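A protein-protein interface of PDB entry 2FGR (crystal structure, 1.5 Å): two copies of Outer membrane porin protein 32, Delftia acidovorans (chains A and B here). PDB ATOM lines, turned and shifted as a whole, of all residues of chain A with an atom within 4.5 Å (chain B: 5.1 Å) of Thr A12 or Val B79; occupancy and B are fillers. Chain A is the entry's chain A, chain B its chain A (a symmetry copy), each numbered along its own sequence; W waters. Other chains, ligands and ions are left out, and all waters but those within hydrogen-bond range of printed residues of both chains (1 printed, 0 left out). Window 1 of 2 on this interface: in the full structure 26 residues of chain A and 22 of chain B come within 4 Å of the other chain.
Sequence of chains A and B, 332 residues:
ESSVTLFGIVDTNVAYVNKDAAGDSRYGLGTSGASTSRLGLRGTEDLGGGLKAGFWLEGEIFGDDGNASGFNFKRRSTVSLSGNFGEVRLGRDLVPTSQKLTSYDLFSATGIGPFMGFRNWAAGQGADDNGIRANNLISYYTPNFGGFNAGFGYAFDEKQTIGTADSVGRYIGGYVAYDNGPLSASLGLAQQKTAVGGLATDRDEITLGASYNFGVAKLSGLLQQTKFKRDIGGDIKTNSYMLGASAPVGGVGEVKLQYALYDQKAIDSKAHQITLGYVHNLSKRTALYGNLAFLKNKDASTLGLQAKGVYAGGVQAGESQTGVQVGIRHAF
Of chain B, only Val B79 (3.9 Å) and Leu B90 (3.9 Å) come within 4 Å of Thr A12.
Of chain A, only Val A10 (3.8 Å), Thr A12 (3.9 Å), Ile A328 (3.6 Å) and His A330 (3.8 Å) come within 4 Å of Val B79.
Of the printed residues of chain A, Ser B77 touches Gly A63.
Of the printed residues of chain B, Gly A63 touches Ser B77 and Gly B91.
Thr A31 touches none of the printed residues of chain B.
The nearest printed residue of chain A that does not touch Val B79 is Asp A11 (5.3 Å).
The nearest printed residue of chain B that does not touch His A330 is Gly B54 (4.4 Å).
Of the 12 printed residues of chain A, 6 touch a printed residue of chain B.
Hydrophobic or aromatic side chains of chain A that line the printed part of chain B: Val A10, Leu A29, Ile A328 and His A330.
Of the 11 printed residues of chain B, 6 touch a printed residue of chain A.
Printed residues of chain B that touch a printed residue of chain A: Phe B55, Ser B77, Val B79, Leu B81, Leu B90 and Gly B91.
Hydrophobic or aromatic side chains of chain B within 4 Å of the printed part of chain A: Phe B55, Val B79, Leu B81 and Leu B90.
Among the printed residues, 11 pairs touch across the chains.
Among the printed residues, merely in contact across the chains: Gly A63 with Gly B91 (3.3 Å), Ile A328 with Val B79 (3.6 Å), Leu A29 with Gly B91 (3.6 Å), His A330 with Phe B55 (3.7 Å), Val A10 with Val B79 (3.8 Å), Ile A328 with Leu B81 (3.8 Å), His A330 with Val B79 (3.8 Å), Thr A12 with Val B79 (3.9 Å), Thr A12 with Leu B90 (3.9 Å) and Ile A328 with Leu B90 (3.9996 Å).
The side-chain hydroxyl (OG) of Ser B77 lies within hydrogen-bond range of the backbone carbonyl oxygen (O) of Gly A63.
Water W1 lies within hydrogen-bond range of the side-chain hydroxyl (OG1) of Thr A12 (2.8 Å), the backbone carbonyl oxygen (O) of Leu B90 (2.8 Å) and the backbone carbonyl oxygen (O) of Ser B77 (2.8 Å).
No position is printed for both chains.
Of the 11 pairs that touch across the chains among the printed residues, none has its exchanged pair printed and touching as well.
N of His A330 sits at hydrogen-bond distance from O of Val A10, at 2.9 Å.
The backbone NH (N) of Ile A328 sits at hydrogen-bond distance from the backbone carbonyl oxygen (O) of Thr A12.
The backbone carbonyl oxygen of Val B79 sits at hydrogen-bond distance from the backbone NH of Leu B90.
The backbone carbonyl oxygen (O) of Leu B81 sits at hydrogen-bond distance from the backbone NH (N) of Val B88 (2.9 Å).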
ATOM      1  N   VAL A  10     -11.127   8.710   1.114  1.00  0.00           N
ATOM      2  CA  VAL A  10     -10.826   7.567   0.259  1.00  0.00           C
ATOM      3  C   VAL A  10     -12.012   6.602   0.367  1.00  0.00           C
ATOM      4  O   VAL A  10     -12.309   6.050   1.435  1.00  0.00           O
ATOM      5  CB  VAL A  10      -9.506   6.897   0.627  1.00  0.00           C
ATOM      6  CG1 VAL A  10      -9.203   5.799  -0.392  1.00  0.00           C
ATOM      7  CG2 VAL A  10      -8.389   7.878   0.635  1.00  0.00           C
ATOM      8  N   ASP A  11     -12.708   6.431  -0.756  1.00  0.00           N
ATOM      9  CA  ASP A  11     -13.867   5.528  -0.839  1.00  0.00           C
ATOM     10  C   ASP A  11     -13.530   4.562  -1.974  1.00  0.00           C
ATOM     11  O   ASP A  11     -13.412   4.961  -3.135  1.00  0.00           O
ATOM     12  CB  ASP A  11     -15.085   6.344  -1.137  1.00  0.00           C
ATOM     13  CG  ASP A  11     -16.307   5.532  -1.389  1.00  0.00           C
ATOM     14  OD1 ASP A  11     -16.186   4.448  -1.996  1.00  0.00           O
ATOM     15  OD2 ASP A  11     -17.453   5.963  -1.033  1.00  0.00           O
ATOM     16  N   THR A  12     -13.306   3.299  -1.605  1.00  0.00           N
ATOM     17  CA  THR A  12     -12.952   2.243  -2.550  1.00  0.00           C
ATOM     18  C   THR A  12     -13.823   1.028  -2.297  1.00  0.00           C
ATOM     19  O   THR A  12     -14.250   0.781  -1.170  1.00  0.00           O
ATOM     20  CB  THR A  12     -11.447   1.950  -2.377  1.00  0.00           C
ATOM     21  OG1 THR A  12     -10.730   3.173  -2.655  1.00  0.00           O
ATOM     22  CG2 THR A  12     -10.956   0.927  -3.330  1.00  0.00           C
ATOM     23  N   ASN A  13     -14.149   0.313  -3.368  1.00  0.00           N
ATOM     24  CA  ASN A  13     -15.183  -0.718  -3.350  1.00  0.00           C
ATOM     25  C   ASN A  13     -14.799  -1.860  -4.266  1.00  0.00           C
ATOM     26  O   ASN A  13     -13.909  -1.740  -5.106  1.00  0.00           O
ATOM     27  CB  ASN A  13     -16.560  -0.181  -3.730  1.00  0.00           C
ATOM     28  CG  ASN A  13     -16.587   0.556  -5.080  1.00  0.00           C
ATOM     29  OD1 ASN A  13     -16.198   0.005  -6.117  1.00  0.00           O
ATOM     30  ND2 ASN A  13     -17.035   1.819  -5.064  1.00  0.00           N
ATOM     31  N   LEU A  29     -12.278  -3.641  -8.760  1.00  0.00           N
ATOM     32  CA  LEU A  29     -12.100  -2.699  -7.650  1.00  0.00           C
ATOM     33  C   LEU A  29     -12.395  -1.332  -8.231  1.00  0.00           C
ATOM     34  O   LEU A  29     -11.745  -0.895  -9.179  1.00  0.00           O
ATOM     35  CB  LEU A  29     -10.662  -2.738  -7.122  1.00  0.00           C
ATOM     36  CG  LEU A  29     -10.544  -2.135  -5.704  1.00  0.00           C
ATOM     37  CD1 LEU A  29     -10.985  -3.110  -4.624  1.00  0.00           C
ATOM     38  CD2 LEU A  29      -9.113  -1.684  -5.427  1.00  0.00           C
ATOM     39  N   GLY A  30     -13.371  -0.665  -7.665  1.00  0.00           N
ATOM     40  CA  GLY A  30     -13.726   0.677  -8.093  1.00  0.00           C
ATOM     41  C   GLY A  30     -13.644   1.661  -6.944  1.00  0.00           C
ATOM     42  O   GLY A  30     -13.088   1.374  -5.891  1.00  0.00           O
ATOM     43  N   THR A  31     -14.228   2.830  -7.149  1.00  0.00           N
ATOM     44  CA  THR A  31     -14.122   3.935  -6.221  1.00  0.00           C
ATOM     45  C   THR A  31     -15.409   4.687  -6.076  1.00  0.00           C
ATOM     46  O   THR A  31     -16.321   4.614  -6.929  1.00  0.00           O
ATOM     47  CB  THR A  31     -13.020   4.941  -6.606  1.00  0.00           C
ATOM     48  OG1 THR A  31     -13.300   5.525  -7.881  1.00  0.00           O
ATOM     49  CG2 THR A  31     -11.688   4.244  -6.778  1.00  0.00           C
ATOM     50  N   GLY A  63      -8.435   5.584  -5.945  1.00  0.00           N
ATOM     51  CA  GLY A  63      -7.592   4.689  -5.165  1.00  0.00           C
ATOM     52  C   GLY A  63      -7.289   3.376  -5.833  1.00  0.00           C
ATOM     53  O   GLY A  63      -6.281   2.727  -5.542  1.00  0.00           O
ATOM     54  N   TYR A 289     -20.362   0.279   3.241  1.00  0.00           N
ATOM     55  CA  TYR A 289     -21.591   0.515   2.511  1.00  0.00           C
ATOM     56  C   TYR A 289     -21.826  -0.515   1.421  1.00  0.00           C
ATOM     57  O   TYR A 289     -20.887  -1.219   0.965  1.00  0.00           O
ATOM     58  CB  TYR A 289     -21.604   1.922   1.886  1.00  0.00           C
ATOM     59  CG  TYR A 289     -20.588   2.104   0.788  1.00  0.00           C
ATOM     60  CD1 TYR A 289     -19.301   2.577   1.064  1.00  0.00           C
ATOM     61  CD2 TYR A 289     -20.873   1.752  -0.511  1.00  0.00           C
ATOM     62  CE1 TYR A 289     -18.356   2.732   0.065  1.00  0.00           C
ATOM     63  CE2 TYR A 289     -19.941   1.886  -1.505  1.00  0.00           C
ATOM     64  CZ  TYR A 289     -18.679   2.398  -1.220  1.00  0.00           C
ATOM     65  OH  TYR A 289     -17.778   2.548  -2.233  1.00  0.00           O
ATOM     66  N   GLY A 327     -18.199  -1.439  -0.286  1.00  0.00           N
ATOM     67  CA  GLY A 327     -16.950  -0.774  -0.006  1.00  0.00           C
ATOM     68  C   GLY A 327     -16.838  -0.111   1.334  1.00  0.00           C
ATOM     69  O   GLY A 327     -17.670  -0.309   2.226  1.00  0.00           O
ATOM     70  N   ILE A 328     -15.775   0.682   1.441  1.00  0.00           N
ATOM     71  CA  ILE A 328     -15.457   1.420   2.628  1.00  0.00           C
ATOM     72  C   ILE A 328     -15.199   2.862   2.228  1.00  0.00           C
ATOM     73  O   ILE A 328     -14.570   3.130   1.202  1.00  0.00           O
ATOM     74  CB  ILE A 328     -14.214   0.821   3.360  1.00  0.00           C
ATOM     75  CG1 ILE A 328     -13.909   1.626   4.625  1.00  0.00           C
ATOM     76  CG2 ILE A 328     -13.008   0.753   2.471  1.00  0.00           C
ATOM     77  CD1 ILE A 328     -13.017   0.833   5.594  1.00  0.00           C
ATOM     78  N   HIS A 330     -13.675   6.308   3.969  1.00  0.00           N
ATOM     79  CA  HIS A 330     -12.923   6.892   5.056  1.00  0.00           C
ATOM     80  C   HIS A 330     -12.610   8.341   4.834  1.00  0.00           C
ATOM     81  O   HIS A 330     -11.869   8.690   3.924  1.00  0.00           O
ATOM     82  CB  HIS A 330     -11.643   6.151   5.291  1.00  0.00           C
ATOM     83  CG  HIS A 330     -10.921   6.623   6.502  1.00  0.00           C
ATOM     84  ND1 HIS A 330      -9.718   7.293   6.464  1.00  0.00           N
ATOM     85  CD2 HIS A 330     -11.311   6.623   7.791  1.00  0.00           C
ATOM     86  CE1 HIS A 330      -9.355   7.590   7.709  1.00  0.00           C
ATOM     87  NE2 HIS A 330     -10.330   7.233   8.522  1.00  0.00           N
ATOM     88  N   GLY B  54      -7.368   3.028   8.236  1.00  0.00           N
ATOM     89  CA  GLY B  54      -6.215   3.727   7.718  1.00  0.00           C
ATOM     90  C   GLY B  54      -6.439   4.202   6.275  1.00  0.00           C
ATOM     91  O   GLY B  54      -7.275   3.708   5.560  1.00  0.00           O
ATOM     92  N   PHE B  55      -5.651   5.190   5.872  1.00  0.00           N
ATOM     93  CA  PHE B  55      -5.504   5.559   4.466  1.00  0.00           C
ATOM     94  C   PHE B  55      -4.041   5.903   4.227  1.00  0.00           C
ATOM     95  O   PHE B  55      -3.298   6.259   5.148  1.00  0.00           O
ATOM     96  CB  PHE B  55      -6.418   6.732   4.083  1.00  0.00           C
ATOM     97  CG  PHE B  55      -5.973   8.059   4.624  1.00  0.00           C
ATOM     98  CD1 PHE B  55      -5.161   8.899   3.888  1.00  0.00           C
ATOM     99  CD2 PHE B  55      -6.278   8.439   5.916  1.00  0.00           C
ATOM    100  CE1 PHE B  55      -4.739  10.099   4.411  1.00  0.00           C
ATOM    101  CE2 PHE B  55      -5.824   9.626   6.437  1.00  0.00           C
ATOM    102  CZ  PHE B  55      -5.036  10.438   5.693  1.00  0.00           C
ATOM    103  N   SER B  77      -2.149   3.957  -2.863  1.00  0.00           N
ATOM    104  CA  SER B  77      -3.378   4.732  -2.678  1.00  0.00           C
ATOM    105  C   SER B  77      -4.427   3.821  -2.079  1.00  0.00           C
ATOM    106  O   SER B  77      -5.344   3.389  -2.758  1.00  0.00           O
ATOM    107  CB  SER B  77      -3.839   5.349  -4.011  1.00  0.00           C
ATOM    108  OG  SER B  77      -4.062   4.368  -5.011  1.00  0.00           O
ATOM    109  N   THR B  78      -4.263   3.535  -0.804  1.00  0.00           N
ATOM    110  CA  THR B  78      -5.065   2.565  -0.111  1.00  0.00           C
ATOM    111  C   THR B  78      -5.940   3.125   0.981  1.00  0.00           C
ATOM    112  O   THR B  78      -5.675   4.199   1.566  1.00  0.00           O
ATOM    113  CB  THR B  78      -4.181   1.454   0.519  1.00  0.00           C
ATOM    114  OG1 THR B  78      -3.205   2.037   1.402  1.00  0.00           O
ATOM    115  CG2 THR B  78      -3.448   0.671  -0.560  1.00  0.00           C
ATOM    116  N   VAL B  79      -6.971   2.332   1.276  1.00  0.00           N
ATOM    117  CA  VAL B  79      -7.749   2.464   2.492  1.00  0.00           C
ATOM    118  C   VAL B  79      -7.763   1.081   3.122  1.00  0.00           C
ATOM    119  O   VAL B  79      -7.754   0.060   2.423  1.00  0.00           O
ATOM    120  CB  VAL B  79      -9.180   3.024   2.194  1.00  0.00           C
ATOM    121  CG1 VAL B  79      -9.957   2.170   1.167  1.00  0.00           C
ATOM    122  CG2 VAL B  79     -10.016   3.169   3.496  1.00  0.00           C
ATOM    123  N   SER B  80      -7.738   1.038   4.442  1.00  0.00           N
ATOM    124  CA  SER B  80      -7.567  -0.217   5.142  1.00  0.00           C
ATOM    125  C   SER B  80      -8.286  -0.291   6.455  1.00  0.00           C
ATOM    126  O   SER B  80      -8.674   0.726   7.025  1.00  0.00           O
ATOM    127  CB  SER B  80      -6.102  -0.448   5.434  1.00  0.00           C
ATOM    128  OG  SER B  80      -5.608   0.597   6.232  1.00  0.00           O
ATOM    129  N   LEU B  81      -8.496  -1.528   6.901  1.00  0.00           N
ATOM    130  CA  LEU B  81      -8.958  -1.811   8.245  1.00  0.00           C
ATOM    131  C   LEU B  81      -7.953  -2.769   8.841  1.00  0.00           C
ATOM    132  O   LEU B  81      -7.528  -3.717   8.159  1.00  0.00           O
ATOM    133  CB  LEU B  81     -10.356  -2.459   8.206  1.00  0.00           C
ATOM    134  CG  LEU B  81     -11.614  -1.818   8.701  1.00  0.00           C
ATOM    135  CD1 LEU B  81     -11.618  -0.334   8.940  1.00  0.00           C
ATOM    136  CD2 LEU B  81     -12.834  -2.378   7.979  1.00  0.00           C
ATOM    137  N   VAL B  88      -6.391  -5.550   6.178  1.00  0.00           N
ATOM    138  CA  VAL B  88      -6.898  -5.660   4.815  1.00  0.00           C
ATOM    139  C   VAL B  88      -6.773  -4.276   4.161  1.00  0.00           C
ATOM    140  O   VAL B  88      -7.204  -3.263   4.734  1.00  0.00           O
ATOM    141  CB  VAL B  88      -8.361  -6.113   4.773  1.00  0.00           C
ATOM    142  CG1 VAL B  88      -8.875  -6.129   3.361  1.00  0.00           C
ATOM    143  CG2 VAL B  88      -8.528  -7.494   5.375  1.00  0.00           C
ATOM    144  N   ARG B  89      -6.168  -4.234   2.978  1.00  0.00           N
ATOM    145  CA  ARG B  89      -5.987  -2.972   2.238  1.00  0.00           C
ATOM    146  C   ARG B  89      -6.630  -3.080   0.881  1.00  0.00           C
ATOM    147  O   ARG B  89      -6.456  -4.102   0.202  1.00  0.00           O
ATOM    148  CB  ARG B  89      -4.525  -2.682   1.955  1.00  0.00           C
ATOM    149  CG  ARG B  89      -3.613  -2.576   3.095  1.00  0.00           C
ATOM    150  CD  ARG B  89      -2.182  -2.163   2.619  1.00  0.00           C
ATOM    151  NE  ARG B  89      -1.276  -2.368   3.697  1.00  0.00           N
ATOM    152  CZ  ARG B  89       0.011  -2.398   3.598  1.00  0.00           C
ATOM    153  NH1 ARG B  89       0.636  -2.286   2.426  1.00  0.00           N
ATOM    154  NH2 ARG B  89       0.677  -2.543   4.716  1.00  0.00           N
ATOM    155  N   LEU B  90      -7.301  -2.015   0.463  1.00  0.00           N
ATOM    156  CA  LEU B  90      -7.864  -1.891  -0.873  1.00  0.00           C
ATOM    157  C   LEU B  90      -7.170  -0.734  -1.586  1.00  0.00           C
ATOM    158  O   LEU B  90      -7.179   0.382  -1.077  1.00  0.00           O
ATOM    159  CB  LEU B  90      -9.373  -1.569  -0.812  1.00  0.00           C
ATOM    160  CG  LEU B  90     -10.466  -2.602  -0.623  1.00  0.00           C
ATOM    161  CD1 LEU B  90     -10.102  -3.736   0.128  1.00  0.00           C
ATOM    162  CD2 LEU B  90     -11.733  -1.983  -0.153  1.00  0.00           C
ATOM    163  N   GLY B  91      -6.711  -0.967  -2.805  1.00  0.00           N
ATOM    164  CA  GLY B  91      -6.160   0.077  -3.650  1.00  0.00           C
ATOM    165  C   GLY B  91      -4.799  -0.307  -4.188  1.00  0.00           C
ATOM    166  O   GLY B  91      -4.160  -1.293  -3.740  1.00  0.00           O
HETATM  167  O   HOH W   1      -8.035   2.753  -2.246  1.00  0.00           O
